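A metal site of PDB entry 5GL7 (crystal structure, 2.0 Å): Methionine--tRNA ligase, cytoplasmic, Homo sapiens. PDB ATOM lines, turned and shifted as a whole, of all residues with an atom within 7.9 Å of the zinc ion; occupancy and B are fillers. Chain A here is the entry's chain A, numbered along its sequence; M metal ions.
The backbone NH (N) of Cys 187 lies within hydrogen-bond range of the backbone carbonyl oxygen (O) of Tyr 192, at 2.7 Å. SG of Cys 187 sits close to N of Phe 189 (3.3 Å). The side-chain sulfur of Cys 190 sits close to the backbone NH of Tyr 192 (3.5 Å). N of Lys 205 sits close to SG of Cys 203 (3.7 Å). The side-chain sulfur (SG) of Cys 200 lies close to the backbone NH (N) of Lys 202 (3.5 Å). N of Cys 200 lies within hydrogen-bond range of O of Lys 205 (3.1 Å).
Four residues have an atom within 4 Å of the zinc ion: Cys 187, Cys 190, Cys 200 and Cys 203. The nearest printed residue that does not touch the zinc ion is Tyr 192 (4.4 Å).
The zinc ion is bound by SG of Cys 187, SG of Cys 190, SG of Cys 203 and SG of Cys 200. The zinc ion has four donor atoms within binding distance.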
ATOM      1  N   VAL A 186     -11.893  21.543   5.000  1.00  0.00           N
ATOM      2  CA  VAL A 186     -13.073  20.841   5.480  1.00  0.00           C
ATOM      3  C   VAL A 186     -12.673  19.710   6.422  1.00  0.00           C
ATOM      4  O   VAL A 186     -11.785  18.919   6.111  1.00  0.00           O
ATOM      5  CB  VAL A 186     -13.900  20.251   4.312  1.00  0.00           C
ATOM      6  CG1 VAL A 186     -15.196  19.653   4.825  1.00  0.00           C
ATOM      7  CG2 VAL A 186     -14.188  21.334   3.275  1.00  0.00           C
ATOM      8  N   CYS A 187     -13.320  19.654   7.583  1.00  0.00           N
ATOM      9  CA  CYS A 187     -13.041  18.604   8.555  1.00  0.00           C
ATOM     10  C   CYS A 187     -13.494  17.237   8.045  1.00  0.00           C
ATOM     11  O   CYS A 187     -14.656  17.057   7.674  1.00  0.00           O
ATOM     12  CB  CYS A 187     -13.734  18.911   9.886  1.00  0.00           C
ATOM     13  SG  CYS A 187     -13.526  17.632  11.143  1.00  0.00           S
ATOM     14  N   PRO A 188     -12.572  16.270   8.021  1.00  0.00           N
ATOM     15  CA  PRO A 188     -12.873  14.912   7.544  1.00  0.00           C
ATOM     16  C   PRO A 188     -13.605  14.075   8.596  1.00  0.00           C
ATOM     17  O   PRO A 188     -13.797  12.880   8.393  1.00  0.00           O
ATOM     18  CB  PRO A 188     -11.496  14.327   7.261  1.00  0.00           C
ATOM     19  CG  PRO A 188     -10.605  15.011   8.251  1.00  0.00           C
ATOM     20  CD  PRO A 188     -11.146  16.417   8.389  1.00  0.00           C
ATOM     21  N   PHE A 189     -14.019  14.707   9.688  1.00  0.00           N
ATOM     22  CA  PHE A 189     -14.719  13.999  10.755  1.00  0.00           C
ATOM     23  C   PHE A 189     -16.156  14.484  10.909  1.00  0.00           C
ATOM     24  O   PHE A 189     -17.046  13.700  11.250  1.00  0.00           O
ATOM     25  CB  PHE A 189     -13.971  14.146  12.079  1.00  0.00           C
ATOM     26  CG  PHE A 189     -12.663  13.395  12.122  1.00  0.00           C
ATOM     27  CD1 PHE A 189     -12.635  12.035  12.353  1.00  0.00           C
ATOM     28  CD2 PHE A 189     -11.463  14.054  11.924  1.00  0.00           C
ATOM     29  CE1 PHE A 189     -11.439  11.336  12.392  1.00  0.00           C
ATOM     30  CE2 PHE A 189     -10.258  13.373  11.952  1.00  0.00           C
ATOM     31  CZ  PHE A 189     -10.252  12.014  12.185  1.00  0.00           C
ATOM     32  N   CYS A 190     -16.407  15.767  10.662  1.00  0.00           N
ATOM     33  CA  CYS A 190     -17.746  16.322  10.843  1.00  0.00           C
ATOM     34  C   CYS A 190     -18.190  17.213   9.681  1.00  0.00           C
ATOM     35  O   CYS A 190     -19.340  17.660   9.636  1.00  0.00           O
ATOM     36  CB  CYS A 190     -17.817  17.109  12.145  1.00  0.00           C
ATOM     37  SG  CYS A 190     -17.085  18.754  12.075  1.00  0.00           S
ATOM     38  N   GLY A 191     -17.287  17.489   8.744  1.00  0.00           N
ATOM     39  CA  GLY A 191     -17.624  18.259   7.560  1.00  0.00           C
ATOM     40  C   GLY A 191     -17.607  19.768   7.735  1.00  0.00           C
ATOM     41  O   GLY A 191     -17.993  20.491   6.818  1.00  0.00           O
ATOM     42  N   TYR A 192     -17.169  20.233   8.899  1.00  0.00           N
ATOM     43  CA  TYR A 192     -17.034  21.662   9.156  1.00  0.00           C
ATOM     44  C   TYR A 192     -16.117  22.295   8.118  1.00  0.00           C
ATOM     45  O   TYR A 192     -15.024  21.787   7.849  1.00  0.00           O
ATOM     46  CB  TYR A 192     -16.499  21.917  10.564  1.00  0.00           C
ATOM     47  CG  TYR A 192     -16.379  23.372  10.946  1.00  0.00           C
ATOM     48  CD1 TYR A 192     -17.496  24.193  11.003  1.00  0.00           C
ATOM     49  CD2 TYR A 192     -15.143  23.923  11.271  1.00  0.00           C
ATOM     50  CE1 TYR A 192     -17.382  25.534  11.349  1.00  0.00           C
ATOM     51  CE2 TYR A 192     -15.021  25.253  11.614  1.00  0.00           C
ATOM     52  CZ  TYR A 192     -16.140  26.058  11.654  1.00  0.00           C
ATOM     53  OH  TYR A 192     -16.026  27.380  12.005  1.00  0.00           O
ATOM     54  N   GLU A 193     -16.568  23.390   7.515  1.00  0.00           N
ATOM     55  CA  GLU A 193     -15.932  23.938   6.328  1.00  0.00           C
ATOM     56  C   GLU A 193     -14.782  24.889   6.629  1.00  0.00           C
ATOM     57  O   GLU A 193     -14.048  25.301   5.725  1.00  0.00           O
ATOM     58  CB  GLU A 193     -16.974  24.645   5.461  1.00  0.00           C
ATOM     59  CG  GLU A 193     -17.806  23.699   4.608  1.00  0.00           C
ATOM     60  CD  GLU A 193     -19.063  24.356   4.067  1.00  0.00           C
ATOM     61  OE1 GLU A 193     -19.235  25.571   4.267  1.00  0.00           O
ATOM     62  OE2 GLU A 193     -19.889  23.645   3.449  1.00  0.00           O
ATOM     63  N   ALA A 195     -12.280  24.309   9.186  1.00  0.00           N
ATOM     64  CA  ALA A 195     -11.370  23.651  10.112  1.00  0.00           C
ATOM     65  C   ALA A 195      -9.950  24.154   9.914  1.00  0.00           C
ATOM     66  O   ALA A 195      -9.545  24.459   8.788  1.00  0.00           O
ATOM     67  CB  ALA A 195     -11.433  22.143   9.941  1.00  0.00           C
ATOM     68  N   GLN A 199      -6.621  21.703  14.344  1.00  0.00           N
ATOM     69  CA  GLN A 199      -7.816  21.301  15.067  1.00  0.00           C
ATOM     70  C   GLN A 199      -9.093  21.806  14.399  1.00  0.00           C
ATOM     71  O   GLN A 199      -9.100  22.880  13.796  1.00  0.00           O
ATOM     72  CB  GLN A 199      -7.756  21.808  16.513  1.00  0.00           C
ATOM     73  CG  GLN A 199      -8.928  21.391  17.397  1.00  0.00           C
ATOM     74  CD  GLN A 199      -8.812  21.909  18.816  1.00  0.00           C
ATOM     75  OE1 GLN A 199      -8.024  22.823  19.093  1.00  0.00           O
ATOM     76  NE2 GLN A 199      -9.594  21.343  19.723  1.00  0.00           N
ATOM     77  N   CYS A 200     -10.167  21.022  14.491  1.00  0.00           N
ATOM     78  CA  CYS A 200     -11.485  21.479  14.085  1.00  0.00           C
ATOM     79  C   CYS A 200     -12.237  21.991  15.297  1.00  0.00           C
ATOM     80  O   CYS A 200     -12.557  21.236  16.205  1.00  0.00           O
ATOM     81  CB  CYS A 200     -12.265  20.346  13.412  1.00  0.00           C
ATOM     82  SG  CYS A 200     -14.005  20.754  13.123  1.00  0.00           S
ATOM     83  N   ASP A 201     -12.531  23.287  15.308  1.00  0.00           N
ATOM     84  CA  ASP A 201     -13.177  23.918  16.465  1.00  0.00           C
ATOM     85  C   ASP A 201     -14.638  23.509  16.626  1.00  0.00           C
ATOM     86  O   ASP A 201     -15.261  23.798  17.647  1.00  0.00           O
ATOM     87  CB  ASP A 201     -13.076  25.439  16.361  1.00  0.00           C
ATOM     88  CG  ASP A 201     -11.645  25.939  16.439  1.00  0.00           C
ATOM     89  OD1 ASP A 201     -10.868  25.393  17.247  1.00  0.00           O
ATOM     90  OD2 ASP A 201     -11.299  26.878  15.696  1.00  0.00           O
ATOM     91  N   LYS A 202     -15.185  22.839  15.617  1.00  0.00           N
ATOM     92  CA  LYS A 202     -16.581  22.444  15.646  1.00  0.00           C
ATOM     93  C   LYS A 202     -16.794  21.120  16.390  1.00  0.00           C
ATOM     94  O   LYS A 202     -17.621  21.042  17.295  1.00  0.00           O
ATOM     95  CB  LYS A 202     -17.136  22.331  14.222  1.00  0.00           C
ATOM     96  CG  LYS A 202     -18.645  22.201  14.161  1.00  0.00           C
ATOM     97  CD  LYS A 202     -19.354  23.478  14.569  1.00  0.00           C
ATOM     98  CE  LYS A 202     -20.859  23.303  14.568  1.00  0.00           C
ATOM     99  NZ  LYS A 202     -21.544  24.358  15.357  1.00  0.00           N
ATOM    100  N   CYS A 203     -16.035  20.101  16.009  1.00  0.00           N
ATOM    101  CA  CYS A 203     -16.161  18.790  16.657  1.00  0.00           C
ATOM    102  C   CYS A 203     -15.031  18.548  17.651  1.00  0.00           C
ATOM    103  O   CYS A 203     -15.049  17.569  18.402  1.00  0.00           O
ATOM    104  CB  CYS A 203     -16.189  17.669  15.603  1.00  0.00           C
ATOM    105  SG  CYS A 203     -14.608  17.333  14.819  1.00  0.00           S
ATOM    106  N   GLY A 204     -14.047  19.447  17.670  1.00  0.00           N
ATOM    107  CA  GLY A 204     -12.997  19.404  18.669  1.00  0.00           C
ATOM    108  C   GLY A 204     -11.787  18.555  18.302  1.00  0.00           C
ATOM    109  O   GLY A 204     -10.741  18.651  18.957  1.00  0.00           O
ATOM    110  N   LYS A 205     -11.926  17.742  17.266  1.00  0.00           N
ATOM    111  CA  LYS A 205     -10.899  16.770  16.906  1.00  0.00           C
ATOM    112  C   LYS A 205      -9.540  17.394  16.589  1.00  0.00           C
ATOM    113  O   LYS A 205      -9.444  18.282  15.740  1.00  0.00           O
ATOM    114  CB  LYS A 205     -11.364  15.941  15.706  1.00  0.00           C
ATOM    115  CG  LYS A 205     -10.495  14.727  15.408  1.00  0.00           C
ATOM    116  CD  LYS A 205     -10.876  13.546  16.282  1.00  0.00           C
ATOM    117  CE  LYS A 205     -10.050  12.314  15.957  1.00  0.00           C
ATOM    118  NZ  LYS A 205     -10.692  11.065  16.456  1.00  0.00           N
ATOM    119  N   ILE A 207      -6.327  17.182  14.635  1.00  0.00           N
ATOM    120  CA  ILE A 207      -6.020  16.531  13.372  1.00  0.00           C
ATOM    121  C   ILE A 207      -4.636  16.909  12.853  1.00  0.00           C
ATOM    122  O   ILE A 207      -3.970  17.784  13.393  1.00  0.00           O
ATOM    123  CB  ILE A 207      -7.042  16.902  12.283  1.00  0.00           C
ATOM    124  CG1 ILE A 207      -7.038  18.421  12.059  1.00  0.00           C
ATOM    125  CG2 ILE A 207      -8.429  16.448  12.680  1.00  0.00           C
ATOM    126  CD1 ILE A 207      -7.556  18.841  10.715  1.00  0.00           C
HETATM  127 ZN    ZN M   1     -14.882  18.537  12.805  1.00  0.00          ZN
